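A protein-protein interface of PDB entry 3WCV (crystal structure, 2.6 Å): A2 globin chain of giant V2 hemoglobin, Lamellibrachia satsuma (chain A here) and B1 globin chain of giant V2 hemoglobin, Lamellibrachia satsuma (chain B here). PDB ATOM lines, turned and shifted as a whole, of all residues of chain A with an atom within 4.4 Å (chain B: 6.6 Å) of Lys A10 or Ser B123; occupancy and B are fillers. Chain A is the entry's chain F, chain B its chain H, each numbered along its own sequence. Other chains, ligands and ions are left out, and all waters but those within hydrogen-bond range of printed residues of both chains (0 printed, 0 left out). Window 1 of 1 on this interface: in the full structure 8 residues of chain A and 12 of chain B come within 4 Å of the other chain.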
ATOM      1  N   LEU A   6      19.330 -28.367  21.056  1.00  0.00           N
ATOM      2  CA  LEU A   6      19.898 -27.751  19.866  1.00  0.00           C
ATOM      3  C   LEU A   6      20.315 -26.308  20.136  1.00  0.00           C
ATOM      4  O   LEU A   6      21.451 -25.928  19.855  1.00  0.00           O
ATOM      5  CB  LEU A   6      18.898 -27.852  18.702  1.00  0.00           C
ATOM      6  CG  LEU A   6      18.444 -29.291  18.360  1.00  0.00           C
ATOM      7  CD1 LEU A   6      17.453 -29.279  17.202  1.00  0.00           C
ATOM      8  CD2 LEU A   6      19.654 -30.160  17.999  1.00  0.00           C
ATOM      9  N   GLN A   7      19.416 -25.513  20.705  1.00  0.00           N
ATOM     10  CA  GLN A   7      19.720 -24.115  21.017  1.00  0.00           C
ATOM     11  C   GLN A   7      20.933 -24.017  21.929  1.00  0.00           C
ATOM     12  O   GLN A   7      21.685 -23.046  21.868  1.00  0.00           O
ATOM     13  CB  GLN A   7      18.538 -23.435  21.707  1.00  0.00           C
ATOM     14  CG  GLN A   7      17.285 -23.291  20.863  1.00  0.00           C
ATOM     15  CD  GLN A   7      16.625 -24.629  20.537  1.00  0.00           C
ATOM     16  OE1 GLN A   7      16.631 -25.567  21.344  1.00  0.00           O
ATOM     17  NE2 GLN A   7      16.029 -24.707  19.358  1.00  0.00           N
ATOM     18  N   ARG A   8      21.122 -25.023  22.772  1.00  0.00           N
ATOM     19  CA  ARG A   8      22.236 -25.022  23.701  1.00  0.00           C
ATOM     20  C   ARG A   8      23.554 -25.305  22.997  1.00  0.00           C
ATOM     21  O   ARG A   8      24.606 -24.806  23.401  1.00  0.00           O
ATOM     22  CB  ARG A   8      21.991 -26.043  24.824  1.00  0.00           C
ATOM     23  CG  ARG A   8      20.819 -25.662  25.733  1.00  0.00           C
ATOM     24  CD  ARG A   8      20.448 -26.768  26.708  1.00  0.00           C
ATOM     25  NE  ARG A   8      19.224 -26.458  27.451  1.00  0.00           N
ATOM     26  CZ  ARG A   8      19.178 -26.168  28.750  1.00  0.00           C
ATOM     27  NH1 ARG A   8      20.289 -26.152  29.483  1.00  0.00           N
ATOM     28  NH2 ARG A   8      18.020 -25.877  29.322  1.00  0.00           N
ATOM     29  N   LEU A   9      23.513 -26.112  21.945  1.00  0.00           N
ATOM     30  CA  LEU A   9      24.738 -26.388  21.229  1.00  0.00           C
ATOM     31  C   LEU A   9      25.054 -25.126  20.443  1.00  0.00           C
ATOM     32  O   LEU A   9      26.192 -24.669  20.433  1.00  0.00           O
ATOM     33  CB  LEU A   9      24.552 -27.555  20.268  1.00  0.00           C
ATOM     34  CG  LEU A   9      24.523 -28.960  20.856  1.00  0.00           C
ATOM     35  CD1 LEU A   9      24.275 -29.976  19.734  1.00  0.00           C
ATOM     36  CD2 LEU A   9      25.830 -29.260  21.566  1.00  0.00           C
ATOM     37  N   LYS A  10      24.019 -24.581  19.800  1.00  0.00           N
ATOM     38  CA  LYS A  10      24.125 -23.384  18.984  1.00  0.00           C
ATOM     39  C   LYS A  10      24.744 -22.280  19.811  1.00  0.00           C
ATOM     40  O   LYS A  10      25.760 -21.709  19.426  1.00  0.00           O
ATOM     41  CB  LYS A  10      22.742 -22.933  18.508  1.00  0.00           C
ATOM     42  CG  LYS A  10      22.742 -21.814  17.467  1.00  0.00           C
ATOM     43  CD  LYS A  10      23.022 -22.394  16.083  1.00  0.00           C
ATOM     44  CE  LYS A  10      22.857 -21.364  14.977  1.00  0.00           C
ATOM     45  NZ  LYS A  10      21.441 -21.137  14.644  1.00  0.00           N
ATOM     46  N   VAL A  11      24.125 -22.001  20.960  1.00  0.00           N
ATOM     47  CA  VAL A  11      24.587 -20.964  21.877  1.00  0.00           C
ATOM     48  C   VAL A  11      26.032 -21.224  22.313  1.00  0.00           C
ATOM     49  O   VAL A  11      26.842 -20.293  22.401  1.00  0.00           O
ATOM     50  CB  VAL A  11      23.617 -20.862  23.122  1.00  0.00           C
ATOM     51  CG1 VAL A  11      24.212 -20.024  24.244  1.00  0.00           C
ATOM     52  CG2 VAL A  11      22.326 -20.219  22.685  1.00  0.00           C
ATOM     53  N   LYS A  12      26.354 -22.484  22.581  1.00  0.00           N
ATOM     54  CA  LYS A  12      27.717 -22.858  22.980  1.00  0.00           C
ATOM     55  C   LYS A  12      28.716 -22.500  21.890  1.00  0.00           C
ATOM     56  O   LYS A  12      29.822 -22.031  22.165  1.00  0.00           O
ATOM     57  CB  LYS A  12      27.820 -24.357  23.233  1.00  0.00           C
ATOM     58  CG  LYS A  12      27.432 -24.802  24.611  1.00  0.00           C
ATOM     59  CD  LYS A  12      27.311 -26.315  24.595  1.00  0.00           C
ATOM     60  CE  LYS A  12      26.982 -26.873  25.958  1.00  0.00           C
ATOM     61  NZ  LYS A  12      28.062 -26.572  26.938  1.00  0.00           N
ATOM     62  N   ARG A  13      28.318 -22.729  20.649  1.00  0.00           N
ATOM     63  CA  ARG A  13      29.190 -22.433  19.537  1.00  0.00           C
ATOM     64  C   ARG A  13      29.340 -20.931  19.327  1.00  0.00           C
ATOM     65  O   ARG A  13      30.457 -20.433  19.317  1.00  0.00           O
ATOM     66  CB  ARG A  13      28.689 -23.108  18.251  1.00  0.00           C
ATOM     67  CG  ARG A  13      29.717 -23.082  17.131  1.00  0.00           C
ATOM     68  CD  ARG A  13      29.385 -24.084  16.040  1.00  0.00           C
ATOM     69  NE  ARG A  13      28.038 -23.845  15.554  1.00  0.00           N
ATOM     70  CZ  ARG A  13      27.669 -22.747  14.905  1.00  0.00           C
ATOM     71  NH1 ARG A  13      26.409 -22.607  14.506  1.00  0.00           N
ATOM     72  NH2 ARG A  13      28.567 -21.808  14.637  1.00  0.00           N
ATOM     73  N   GLN A  14      28.232 -20.214  19.179  1.00  0.00           N
ATOM     74  CA  GLN A  14      28.305 -18.786  18.944  1.00  0.00           C
ATOM     75  C   GLN A  14      28.973 -18.072  20.088  1.00  0.00           C
ATOM     76  O   GLN A  14      29.612 -17.040  19.890  1.00  0.00           O
ATOM     77  CB  GLN A  14      26.922 -18.215  18.684  1.00  0.00           C
ATOM     78  CG  GLN A  14      26.243 -18.902  17.524  1.00  0.00           C
ATOM     79  CD  GLN A  14      25.076 -18.096  16.953  1.00  0.00           C
ATOM     80  OE1 GLN A  14      24.316 -17.471  17.692  1.00  0.00           O
ATOM     81  NE2 GLN A  14      24.927 -18.123  15.629  1.00  0.00           N
ATOM     82  N   ASP A 126      21.815 -15.989  16.245  1.00  0.00           N
ATOM     83  CA  ASP A 126      20.571 -16.716  16.483  1.00  0.00           C
ATOM     84  C   ASP A 126      19.871 -16.157  17.739  1.00  0.00           C
ATOM     85  O   ASP A 126      20.121 -16.600  18.861  1.00  0.00           O
ATOM     86  CB  ASP A 126      20.897 -18.214  16.625  1.00  0.00           C
ATOM     87  CG  ASP A 126      19.661 -19.076  16.659  1.00  0.00           C
ATOM     88  OD1 ASP A 126      19.772 -20.297  16.429  1.00  0.00           O
ATOM     89  OD2 ASP A 126      18.577 -18.523  16.926  1.00  0.00           O
ATOM     90  N   GLN B  18      30.794 -27.163  10.477  1.00  0.00           N
ATOM     91  CA  GLN B  18      30.551 -26.221  11.552  1.00  0.00           C
ATOM     92  C   GLN B  18      30.197 -26.994  12.831  1.00  0.00           C
ATOM     93  O   GLN B  18      30.756 -26.753  13.910  1.00  0.00           O
ATOM     94  CB  GLN B  18      29.362 -25.328  11.222  1.00  0.00           C
ATOM     95  CG  GLN B  18      29.647 -24.085  10.432  1.00  0.00           C
ATOM     96  CD  GLN B  18      28.380 -23.260  10.216  1.00  0.00           C
ATOM     97  OE1 GLN B  18      27.648 -22.970  11.166  1.00  0.00           O
ATOM     98  NE2 GLN B  18      28.116 -22.879   8.965  1.00  0.00           N
ATOM     99  N   THR B 119      14.719 -30.328   9.354  1.00  0.00           N
ATOM    100  CA  THR B 119      14.080 -29.621  10.461  1.00  0.00           C
ATOM    101  C   THR B 119      15.078 -29.370  11.575  1.00  0.00           C
ATOM    102  O   THR B 119      15.079 -28.305  12.187  1.00  0.00           O
ATOM    103  CB  THR B 119      12.893 -30.415  11.075  1.00  0.00           C
ATOM    104  OG1 THR B 119      11.885 -30.649  10.082  1.00  0.00           O
ATOM    105  CG2 THR B 119      12.284 -29.644  12.258  1.00  0.00           C
ATOM    106  N   VAL B 120      15.922 -30.362  11.834  1.00  0.00           N
ATOM    107  CA  VAL B 120      16.906 -30.274  12.904  1.00  0.00           C
ATOM    108  C   VAL B 120      18.124 -29.376  12.619  1.00  0.00           C
ATOM    109  O   VAL B 120      18.435 -28.482  13.398  1.00  0.00           O
ATOM    110  CB  VAL B 120      17.373 -31.703  13.294  1.00  0.00           C
ATOM    111  CG1 VAL B 120      18.565 -31.639  14.221  1.00  0.00           C
ATOM    112  CG2 VAL B 120      16.213 -32.451  13.957  1.00  0.00           C
ATOM    113  N   LEU B 121      18.792 -29.594  11.497  1.00  0.00           N
ATOM    114  CA  LEU B 121      19.963 -28.815  11.146  1.00  0.00           C
ATOM    115  C   LEU B 121      19.892 -27.283  11.237  1.00  0.00           C
ATOM    116  O   LEU B 121      20.812 -26.655  11.764  1.00  0.00           O
ATOM    117  CB  LEU B 121      20.430 -29.211   9.753  1.00  0.00           C
ATOM    118  CG  LEU B 121      20.856 -30.672   9.666  1.00  0.00           C
ATOM    119  CD1 LEU B 121      21.325 -30.981   8.255  1.00  0.00           C
ATOM    120  CD2 LEU B 121      21.966 -30.941  10.687  1.00  0.00           C
ATOM    121  N   PRO B 122      18.831 -26.660  10.708  1.00  0.00           N
ATOM    122  CA  PRO B 122      18.823 -25.201  10.822  1.00  0.00           C
ATOM    123  C   PRO B 122      18.991 -24.663  12.248  1.00  0.00           C
ATOM    124  O   PRO B 122      19.468 -23.542  12.446  1.00  0.00           O
ATOM    125  CB  PRO B 122      17.497 -24.793  10.162  1.00  0.00           C
ATOM    126  CG  PRO B 122      16.726 -26.097   9.978  1.00  0.00           C
ATOM    127  CD  PRO B 122      17.776 -27.129   9.793  1.00  0.00           C
ATOM    128  N   SER B 123      18.626 -25.463  13.242  1.00  0.00           N
ATOM    129  CA  SER B 123      18.758 -25.033  14.629  1.00  0.00           C
ATOM    130  C   SER B 123      20.180 -25.227  15.132  1.00  0.00           C
ATOM    131  O   SER B 123      20.515 -24.781  16.228  1.00  0.00           O
ATOM    132  CB  SER B 123      17.805 -25.822  15.540  1.00  0.00           C
ATOM    133  OG  SER B 123      16.449 -25.551  15.239  1.00  0.00           O
ATOM    134  N   LEU B 124      21.013 -25.905  14.344  1.00  0.00           N
ATOM    135  CA  LEU B 124      22.399 -26.145  14.739  1.00  0.00           C
ATOM    136  C   LEU B 124      23.388 -25.350  13.878  1.00  0.00           C
ATOM    137  O   LEU B 124      24.391 -24.832  14.366  1.00  0.00           O
ATOM    138  CB  LEU B 124      22.718 -27.642  14.640  1.00  0.00           C
ATOM    139  CG  LEU B 124      21.973 -28.630  15.556  1.00  0.00           C
ATOM    140  CD1 LEU B 124      22.146 -30.047  15.044  1.00  0.00           C
ATOM    141  CD2 LEU B 124      22.491 -28.526  16.969  1.00  0.00           C
ATOM    142  N   ILE B 125      23.071 -25.247  12.593  1.00  0.00           N
ATOM    143  CA  ILE B 125      23.919 -24.581  11.612  1.00  0.00           C
ATOM    144  C   ILE B 125      23.674 -23.085  11.396  1.00  0.00           C
ATOM    145  O   ILE B 125      22.533 -22.622  11.348  1.00  0.00           O
ATOM    146  CB  ILE B 125      23.802 -25.332  10.261  1.00  0.00           C
ATOM    147  CG1 ILE B 125      24.410 -26.745  10.415  1.00  0.00           C
ATOM    148  CG2 ILE B 125      24.452 -24.530   9.149  1.00  0.00           C
ATOM    149  CD1 ILE B 125      24.117 -27.701   9.268  1.00  0.00           C
ATOM    150  N   ASP B 126      24.769 -22.333  11.282  1.00  0.00           N
ATOM    151  CA  ASP B 126      24.683 -20.904  11.048  1.00  0.00           C
ATOM    152  C   ASP B 126      24.173 -20.658   9.656  1.00  0.00           C
ATOM    153  O   ASP B 126      24.762 -21.091   8.677  1.00  0.00           O
ATOM    154  CB  ASP B 126      26.041 -20.223  11.190  1.00  0.00           C
ATOM    155  CG  ASP B 126      26.524 -20.170  12.628  1.00  0.00           C
ATOM    156  OD1 ASP B 126      25.686 -20.133  13.567  1.00  0.00           O
ATOM    157  OD2 ASP B 126      27.758 -20.147  12.820  1.00  0.00           O
ATOM    158  N   ASN B 127      23.049 -19.970   9.585  1.00  0.00           N
ATOM    159  CA  ASN B 127      22.451 -19.616   8.323  1.00  0.00           C
ATOM    160  C   ASN B 127      22.391 -20.767   7.345  1.00  0.00           C
ATOM    161  O   ASN B 127      22.963 -20.729   6.262  1.00  0.00           O
ATOM    162  CB  ASN B 127      23.209 -18.441   7.735  1.00  0.00           C
ATOM    163  CG  ASN B 127      22.409 -17.704   6.722  1.00  0.00           C
ATOM    164  OD1 ASN B 127      21.240 -17.368   6.954  1.00  0.00           O
ATOM    165  ND2 ASN B 127      23.024 -17.428   5.587  1.00  0.00           N
ATOM    166  N   PHE B 128      21.662 -21.792   7.768  1.00  0.00           N
ATOM    167  CA  PHE B 128      21.415 -23.016   7.014  1.00  0.00           C
ATOM    168  C   PHE B 128      20.855 -22.721   5.631  1.00  0.00           C
ATOM    169  O   PHE B 128      20.027 -21.831   5.457  1.00  0.00           O
ATOM    170  CB  PHE B 128      20.403 -23.871   7.798  1.00  0.00           C
ATOM    171  CG  PHE B 128      20.119 -25.215   7.185  1.00  0.00           C
ATOM    172  CD1 PHE B 128      21.040 -26.257   7.315  1.00  0.00           C
ATOM    173  CD2 PHE B 128      18.918 -25.446   6.505  1.00  0.00           C
ATOM    174  CE1 PHE B 128      20.772 -27.505   6.785  1.00  0.00           C
ATOM    175  CE2 PHE B 128      18.633 -26.696   5.966  1.00  0.00           C
ATOM    176  CZ  PHE B 128      19.562 -27.728   6.108  1.00  0.00           C
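The guanidinium group (NH1) of Arg A13 is in hydrogen-bond range of the backbone carbonyl oxygen (O) of Leu B124 (3.0 Å).
The side-chain carboxylate (OD2) of Asp B126 is in salt-bridge range of the guanidinium group (NH2) of Arg A13.
NE2 of Gln A14 lies within hydrogen-bond range of OD1 of Asp B126, at 3.0 Å.
The side-chain amino group (NZ) of Lys A10 is in salt-bridge range of the side-chain carboxylate (OD1) of Asp A126 (2.6 Å).
OE1 of Gln A14 is in hydrogen-bond range of N of Asp A126.
The backbone NH (N) of Asp B126 is in hydrogen-bond range of the side-chain amide oxygen (OE1) of Gln B18.
Val B120 touches Leu A6.
Leu A6 touches Ser B123 (CD1 to CB, 3.9 Å).
CD2 of Leu B124 touches CD2 of Leu A6 (3.4 Å).
Leu A9 touches Leu B124.
Lys A10 touches Pro B122 (NZ to O, 3.8 Å).
Lys A10 touches Ser B123.
O of Leu B124 touches CD of Lys A10 (3.3 Å).
Ile B125 touches Lys A10 (O to NZ, 3.8 Å).
Lys A10 touches Asp B126.
Arg A13 touches Gln B18 (NH1 to OE1, 3.6 Å).
Printed residues of chain B within 4 Å of Leu A6: Val B120, Ser B123 and Leu B124.
Gln A7 touches none of the printed residues of chain B.
Printed residues of chain B within 4 Å of Leu A9: Leu B124.
Of chain B, only Pro B122 (3.8 Å), Ser B123 (3.5 Å), Leu B124 (3.3 Å), Ile B125 (3.8 Å) and Asp B126 (3.4 Å) come within 4 Å of Lys A10.
Ser B123 touches just these residues of chain A: Leu A6 and Lys A10.
Of the printed residues of chain A, Leu B124 touches Leu A6 (3.4 Å), Leu A9 (3.6 Å), Lys A10 (3.3 Å) and Arg A13 (3.0 Å).
Of the printed residues of chain A, Ile B125 touches Lys A10.
The nearest printed residue of chain B that does not touch Leu A6 is Thr B119 (5.6 Å).
Hydrophobic or aromatic side chains of chain A within 4 Å of the printed part of chain B: Leu A6 and Leu A9.
Printed residues of chain B that touch a printed residue of chain A: Gln B18, Val B120, Pro B122, Ser B123, Leu B124, Ile B125 and Asp B126.
Hydrophobic or aromatic side chains of chain B that line the printed part of chain A: Val B120 and Leu B124.
Among the printed residues, 13 pairs touch across the chains.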
